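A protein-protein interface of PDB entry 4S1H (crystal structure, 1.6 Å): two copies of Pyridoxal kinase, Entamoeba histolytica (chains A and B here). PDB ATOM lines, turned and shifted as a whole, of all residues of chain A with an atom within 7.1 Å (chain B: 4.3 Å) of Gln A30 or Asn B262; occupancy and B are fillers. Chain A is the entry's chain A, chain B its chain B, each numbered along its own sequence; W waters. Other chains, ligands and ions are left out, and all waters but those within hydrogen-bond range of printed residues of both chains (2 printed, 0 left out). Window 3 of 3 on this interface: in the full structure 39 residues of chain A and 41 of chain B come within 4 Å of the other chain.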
ATOM      1  N   MET A   1      28.614 -21.633 -21.632  1.00  0.00           N
ATOM      2  CA  MET A   1      29.370 -21.050 -22.789  1.00  0.00           C
ATOM      3  C   MET A   1      29.797 -22.133 -23.779  1.00  0.00           C
ATOM      4  O   MET A   1      30.794 -22.825 -23.561  1.00  0.00           O
ATOM      5  CB  MET A   1      30.634 -20.324 -22.317  1.00  0.00           C
ATOM      6  CG  MET A   1      30.426 -18.985 -21.637  1.00  0.00           C
ATOM      7  SD  MET A   1      32.032 -18.356 -21.075  1.00  0.00           S
ATOM      8  CE  MET A   1      32.804 -17.918 -22.638  1.00  0.00           C
ATOM      9  N   THR A   2      29.050 -22.268 -24.864  1.00  0.00           N
ATOM     10  CA  THR A   2      29.388 -23.211 -25.932  1.00  0.00           C
ATOM     11  C   THR A   2      29.495 -22.482 -27.269  1.00  0.00           C
ATOM     12  O   THR A   2      28.724 -21.567 -27.549  1.00  0.00           O
ATOM     13  CB  THR A   2      28.325 -24.300 -26.050  1.00  0.00           C
ATOM     14  OG1 THR A   2      27.072 -23.701 -26.341  1.00  0.00           O
ATOM     15  CG2 THR A   2      28.209 -25.072 -24.701  1.00  0.00           C
ATOM     16  N   ILE A  24      33.205  -9.129 -36.155  1.00  0.00           N
ATOM     17  CA  ILE A  24      32.502  -7.922 -35.801  1.00  0.00           C
ATOM     18  C   ILE A  24      31.000  -8.204 -35.708  1.00  0.00           C
ATOM     19  O   ILE A  24      30.337  -7.786 -34.759  1.00  0.00           O
ATOM     20  CB  ILE A  24      32.764  -6.796 -36.822  1.00  0.00           C
ATOM     21  CG1 ILE A  24      34.223  -6.350 -36.727  1.00  0.00           C
ATOM     22  CG2 ILE A  24      31.828  -5.605 -36.586  1.00  0.00           C
ATOM     23  CD1 ILE A  24      34.694  -5.583 -37.953  1.00  0.00           C
ATOM     24  N   ILE A  25      30.469  -8.904 -36.709  1.00  0.00           N
ATOM     25  CA  ILE A  25      29.025  -9.102 -36.799  1.00  0.00           C
ATOM     26  C   ILE A  25      28.540 -10.116 -35.742  1.00  0.00           C
ATOM     27  O   ILE A  25      27.613  -9.829 -34.981  1.00  0.00           O
ATOM     28  CB  ILE A  25      28.583  -9.475 -38.228  1.00  0.00           C
ATOM     29  CG1 ILE A  25      28.951  -8.314 -39.144  1.00  0.00           C
ATOM     30  CG2 ILE A  25      27.096  -9.785 -38.242  1.00  0.00           C
ATOM     31  CD1 ILE A  25      29.012  -8.660 -40.622  1.00  0.00           C
ATOM     32  N   LEU A  26      29.143 -11.291 -35.722  1.00  0.00           N
ATOM     33  CA  LEU A  26      28.751 -12.339 -34.756  1.00  0.00           C
ATOM     34  C   LEU A  26      29.000 -11.891 -33.316  1.00  0.00           C
ATOM     35  O   LEU A  26      28.154 -12.140 -32.443  1.00  0.00           O
ATOM     36  CB  LEU A  26      29.447 -13.659 -35.060  1.00  0.00           C
ATOM     37  CG  LEU A  26      28.990 -14.365 -36.336  1.00  0.00           C
ATOM     38  CD1 LEU A  26      29.944 -15.462 -36.776  1.00  0.00           C
ATOM     39  CD2 LEU A  26      27.579 -14.925 -36.202  1.00  0.00           C
ATOM     40  N   ASP A  27      30.097 -11.193 -33.069  1.00  0.00           N
ATOM     41  CA  ASP A  27      30.301 -10.598 -31.717  1.00  0.00           C
ATOM     42  C   ASP A  27      29.143  -9.622 -31.356  1.00  0.00           C
ATOM     43  O   ASP A  27      28.591  -9.677 -30.246  1.00  0.00           O
ATOM     44  CB  ASP A  27      31.669  -9.866 -31.553  1.00  0.00           C
ATOM     45  CG  ASP A  27      32.919 -10.806 -31.650  1.00  0.00           C
ATOM     46  OD1 ASP A  27      32.807 -12.061 -31.631  1.00  0.00           O
ATOM     47  OD2 ASP A  27      34.062 -10.262 -31.775  1.00  0.00           O
ATOM     48  N   SER A  28      28.736  -8.756 -32.285  1.00  0.00           N
ATOM     49  CA  SER A  28      27.687  -7.786 -32.007  1.00  0.00           C
ATOM     50  C   SER A  28      26.310  -8.442 -31.769  1.00  0.00           C
ATOM     51  O   SER A  28      25.493  -7.915 -31.041  1.00  0.00           O
ATOM     52  CB  SER A  28      27.596  -6.707 -33.105  1.00  0.00           C
ATOM     53  OG  SER A  28      26.329  -6.720 -33.741  1.00  0.00           O
ATOM     54  N   PHE A  29      26.099  -9.615 -32.359  1.00  0.00           N
ATOM     55  CA  PHE A  29      24.875 -10.404 -32.126  1.00  0.00           C
ATOM     56  C   PHE A  29      25.017 -11.330 -30.916  1.00  0.00           C
ATOM     57  O   PHE A  29      24.083 -12.031 -30.594  1.00  0.00           O
ATOM     58  CB  PHE A  29      24.501 -11.257 -33.374  1.00  0.00           C
ATOM     59  CG  PHE A  29      23.678 -10.540 -34.428  1.00  0.00           C
ATOM     60  CD1 PHE A  29      24.274  -9.751 -35.388  1.00  0.00           C
ATOM     61  CD2 PHE A  29      22.279 -10.715 -34.495  1.00  0.00           C
ATOM     62  CE1 PHE A  29      23.524  -9.107 -36.351  1.00  0.00           C
ATOM     63  CE2 PHE A  29      21.517 -10.074 -35.468  1.00  0.00           C
ATOM     64  CZ  PHE A  29      22.142  -9.263 -36.402  1.00  0.00           C
ATOM     65  N   GLN A  30      26.201 -11.349 -30.288  1.00  0.00           N
ATOM     66  CA  GLN A  30      26.506 -12.180 -29.142  1.00  0.00           C
ATOM     67  C   GLN A  30      26.280 -13.671 -29.425  1.00  0.00           C
ATOM     68  O   GLN A  30      25.781 -14.417 -28.583  1.00  0.00           O
ATOM     69  CB  GLN A  30      25.752 -11.697 -27.912  1.00  0.00           C
ATOM     70  CG  GLN A  30      26.141 -10.264 -27.532  1.00  0.00           C
ATOM     71  CD  GLN A  30      25.173  -9.695 -26.562  1.00  0.00           C
ATOM     72  OE1 GLN A  30      24.127  -9.215 -26.961  1.00  0.00           O
ATOM     73  NE2 GLN A  30      25.498  -9.763 -25.275  1.00  0.00           N
ATOM     74  N   ILE A  31      26.761 -14.081 -30.578  1.00  0.00           N
ATOM     75  CA  ILE A  31      26.729 -15.481 -31.031  1.00  0.00           C
ATOM     76  C   ILE A  31      28.166 -16.014 -30.854  1.00  0.00           C
ATOM     77  O   ILE A  31      29.102 -15.572 -31.529  1.00  0.00           O
ATOM     78  CB  ILE A  31      26.217 -15.596 -32.476  1.00  0.00           C
ATOM     79  CG1 ILE A  31      24.749 -15.086 -32.603  1.00  0.00           C
ATOM     80  CG2 ILE A  31      26.348 -17.042 -32.928  1.00  0.00           C
ATOM     81  CD1 ILE A  31      24.258 -14.890 -34.024  1.00  0.00           C
ATOM     82  N   GLN A  32      28.344 -16.898 -29.875  1.00  0.00           N
ATOM     83  CA  GLN A  32      29.676 -17.406 -29.573  1.00  0.00           C
ATOM     84  C   GLN A  32      30.154 -18.270 -30.740  1.00  0.00           C
ATOM     85  O   GLN A  32      29.468 -19.222 -31.143  1.00  0.00           O
ATOM     86  CB  GLN A  32      29.679 -18.201 -28.288  1.00  0.00           C
ATOM     87  CG  GLN A  32      31.089 -18.611 -27.916  1.00  0.00           C
ATOM     88  CD  GLN A  32      31.213 -19.183 -26.526  1.00  0.00           C
ATOM     89  OE1 GLN A  32      30.667 -18.632 -25.572  1.00  0.00           O
ATOM     90  NE2 GLN A  32      31.949 -20.283 -26.397  1.00  0.00           N
ATOM     91  N   SER A  33      31.322 -17.922 -31.287  1.00  0.00           N
ATOM     92  CA  SER A  33      31.818 -18.517 -32.538  1.00  0.00           C
ATOM     93  C   SER A  33      33.315 -18.812 -32.490  1.00  0.00           C
ATOM     94  O   SER A  33      34.055 -18.155 -31.749  1.00  0.00           O
ATOM     95  CB  SER A  33      31.530 -17.571 -33.689  1.00  0.00           C
ATOM     96  OG  SER A  33      30.144 -17.251 -33.716  1.00  0.00           O
ATOM     97  N   LYS A 230      19.123 -16.546 -35.049  1.00  0.00           N
ATOM     98  CA  LYS A 230      18.106 -16.002 -34.136  1.00  0.00           C
ATOM     99  C   LYS A 230      16.670 -16.512 -34.419  1.00  0.00           C
ATOM    100  O   LYS A 230      15.742 -16.156 -33.684  1.00  0.00           O
ATOM    101  CB  LYS A 230      18.148 -14.467 -34.136  1.00  0.00           C
ATOM    102  CG  LYS A 230      19.462 -13.833 -33.644  1.00  0.00           C
ATOM    103  CD  LYS A 230      19.723 -14.072 -32.182  1.00  0.00           C
ATOM    104  CE  LYS A 230      21.105 -13.555 -31.808  1.00  0.00           C
ATOM    105  NZ  LYS A 230      21.392 -13.838 -30.376  1.00  0.00           N
ATOM    106  N   LYS A 268      22.039  -5.083 -35.775  1.00  0.00           N
ATOM    107  CA  LYS A 268      20.859  -5.819 -35.325  1.00  0.00           C
ATOM    108  C   LYS A 268      19.562  -5.129 -35.701  1.00  0.00           C
ATOM    109  O   LYS A 268      18.495  -5.461 -35.177  1.00  0.00           O
ATOM    110  CB  LYS A 268      20.892  -6.035 -33.801  1.00  0.00           C
ATOM    111  CG  LYS A 268      21.954  -7.013 -33.328  1.00  0.00           C
ATOM    112  CD  LYS A 268      21.888  -7.272 -31.821  1.00  0.00           C
ATOM    113  CE  LYS A 268      20.548  -7.804 -31.335  1.00  0.00           C
ATOM    114  NZ  LYS A 268      19.847  -8.858 -32.142  1.00  0.00           N
ATOM    115  N   ASN B 259      33.485 -14.911 -19.764  1.00  0.00           N
ATOM    116  CA  ASN B 259      32.206 -14.724 -20.493  1.00  0.00           C
ATOM    117  C   ASN B 259      32.079 -13.342 -21.174  1.00  0.00           C
ATOM    118  O   ASN B 259      31.071 -12.631 -21.036  1.00  0.00           O
ATOM    119  CB  ASN B 259      31.051 -14.961 -19.522  1.00  0.00           C
ATOM    120  CG  ASN B 259      29.729 -15.243 -20.209  1.00  0.00           C
ATOM    121  OD1 ASN B 259      29.691 -15.507 -21.401  1.00  0.00           O
ATOM    122  ND2 ASN B 259      28.654 -15.173 -19.459  1.00  0.00           N
ATOM    123  N   ILE B 260      33.077 -12.989 -21.968  1.00  0.00           N
ATOM    124  CA  ILE B 260      33.164 -11.648 -22.527  1.00  0.00           C
ATOM    125  C   ILE B 260      32.123 -11.393 -23.655  1.00  0.00           C
ATOM    126  O   ILE B 260      31.592 -10.294 -23.727  1.00  0.00           O
ATOM    127  CB  ILE B 260      34.600 -11.299 -22.951  1.00  0.00           C
ATOM    128  CG1 ILE B 260      34.715  -9.801 -23.231  1.00  0.00           C
ATOM    129  CG2 ILE B 260      35.021 -12.101 -24.184  1.00  0.00           C
ATOM    130  CD1 ILE B 260      36.134  -9.355 -23.521  1.00  0.00           C
ATOM    131  N   ILE B 261      31.787 -12.410 -24.469  1.00  0.00           N
ATOM    132  CA  ILE B 261      30.789 -12.235 -25.580  1.00  0.00           C
ATOM    133  C   ILE B 261      29.416 -11.849 -25.050  1.00  0.00           C
ATOM    134  O   ILE B 261      28.830 -10.839 -25.451  1.00  0.00           O
ATOM    135  CB  ILE B 261      30.655 -13.483 -26.479  1.00  0.00           C
ATOM    136  CG1 ILE B 261      31.981 -13.795 -27.158  1.00  0.00           C
ATOM    137  CG2 ILE B 261      29.607 -13.253 -27.572  1.00  0.00           C
ATOM    138  CD1 ILE B 261      32.538 -12.699 -28.051  1.00  0.00           C
ATOM    139  N   ASN B 262      28.925 -12.599 -24.069  1.00  0.00           N
ATOM    140  CA  ASN B 262      27.664 -12.274 -23.436  1.00  0.00           C
ATOM    141  C   ASN B 262      27.632 -10.964 -22.671  1.00  0.00           C
ATOM    142  O   ASN B 262      26.571 -10.375 -22.499  1.00  0.00           O
ATOM    143  CB  ASN B 262      27.152 -13.468 -22.639  1.00  0.00           C
ATOM    144  CG  ASN B 262      26.858 -14.673 -23.551  1.00  0.00           C
ATOM    145  OD1 ASN B 262      26.127 -14.544 -24.546  1.00  0.00           O
ATOM    146  ND2 ASN B 262      27.456 -15.834 -23.253  1.00  0.00           N
ATOM    147  N   CYS B 263      28.802 -10.520 -22.227  1.00  0.00           N
ATOM    148  CA  CYS B 263      28.990  -9.276 -21.470  1.00  0.00           C
ATOM    149  C   CYS B 263      29.296  -8.070 -22.341  1.00  0.00           C
ATOM    150  O   CYS B 263      29.447  -6.969 -21.816  1.00  0.00           O
ATOM    151  CB  CYS B 263      30.083  -9.444 -20.393  1.00  0.00           C
ATOM    152  SG  CYS B 263      29.515 -10.561 -19.118  1.00  0.00           S
ATOM    153  N   ILE B 264      29.297  -8.234 -23.675  1.00  0.00           N
ATOM    154  CA  ILE B 264      29.583  -7.106 -24.557  1.00  0.00           C
ATOM    155  C   ILE B 264      28.751  -5.861 -24.230  1.00  0.00           C
ATOM    156  O   ILE B 264      29.325  -4.781 -24.193  1.00  0.00           O
ATOM    157  CB  ILE B 264      29.491  -7.501 -26.063  1.00  0.00           C
ATOM    158  CG1 ILE B 264      30.735  -8.249 -26.502  1.00  0.00           C
ATOM    159  CG2 ILE B 264      29.235  -6.282 -26.970  1.00  0.00           C
ATOM    160  CD1 ILE B 264      30.589  -8.977 -27.841  1.00  0.00           C
ATOM    161  N   PRO B 265      27.428  -6.000 -23.963  1.00  0.00           N
ATOM    162  CA  PRO B 265      26.589  -4.851 -23.643  1.00  0.00           C
ATOM    163  C   PRO B 265      26.982  -4.018 -22.420  1.00  0.00           C
ATOM    164  O   PRO B 265      26.531  -2.877 -22.276  1.00  0.00           O
ATOM    165  CB  PRO B 265      25.200  -5.481 -23.434  1.00  0.00           C
ATOM    166  CG  PRO B 265      25.206  -6.671 -24.312  1.00  0.00           C
ATOM    167  CD  PRO B 265      26.612  -7.200 -24.198  1.00  0.00           C
HETATM  168  O   HOH W   1      24.007 -10.814 -23.429  1.00  0.00           O
HETATM  169  O   HOH W   2      25.820 -16.447 -26.594  1.00  0.00           O
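Water W1 lies within hydrogen-bond range of NE2 of Gln A30 (2.6 Å) and O of Asn B262 (2.8 Å).
Water W2 bridges OD1 of Asn B262 (2.8 Å) and O of Gln A30 (2.8 Å).
No position is printed for both chains.
Ile A25 touches none of the printed residues of chain B.
Of the printed residues of chain B, Asp A27 touches Ile B261 (3.6 Å) and Ile B264 (3.2 Å).
Of chain B, only Ile B261 (3.4 Å), Asn B262 (3.0 Å) and Pro B265 (3.0 Å) come within 4 Å of Gln A30.
Of the printed residues of chain A, Ile B261 touches Asp A27 (3.6 Å) and Gln A30 (3.4 Å).
Of chain A, only Gln A30 (3.0 Å) comes within 4 Å of Asn B262.
Of the printed residues of chain A, Pro B265 touches Gln A30 (3.0 Å).
The nearest residue of chain A that does not touch Asn B262 is Met A1 (4.6 Å).
The nearest printed residue of chain B that does not touch Met A1 is Asn B262 (4.6 Å).
The side-chain amide nitrogen of Asn B262 sits at hydrogen-bond distance from the side-chain amide oxygen of Asn B259.
The backbone carbonyl oxygen of Asn B259 sits at hydrogen-bond distance from the side-chain sulfur of Cys B263.
The backbone carbonyl oxygen (O) of Asn B262 lies within hydrogen-bond range of the side-chain amide nitrogen (NE2) of Gln A30, at 3.0 Å.
SD of Met A1 lies close to OD1 of Asn B259, at 3.7 Å.
Of the 7 printed residues of chain B, 5 touch a printed residue of chain A.
Of the 14 printed residues of chain A, 3 touch a printed residue of chain B.
Hydrophobic or aromatic side chains of chain A that line the printed part of chain B: Met A1.
OD1 of Asp A27 touches CD1 of Ile B261, at 3.6 Å.
Ile B264 touches Asp A27 (CD1 to O, 3.2 Å).
O of Ile B261 touches CG of Gln A30, 3.4 Å away.
Gln A30 touches Pro B265.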
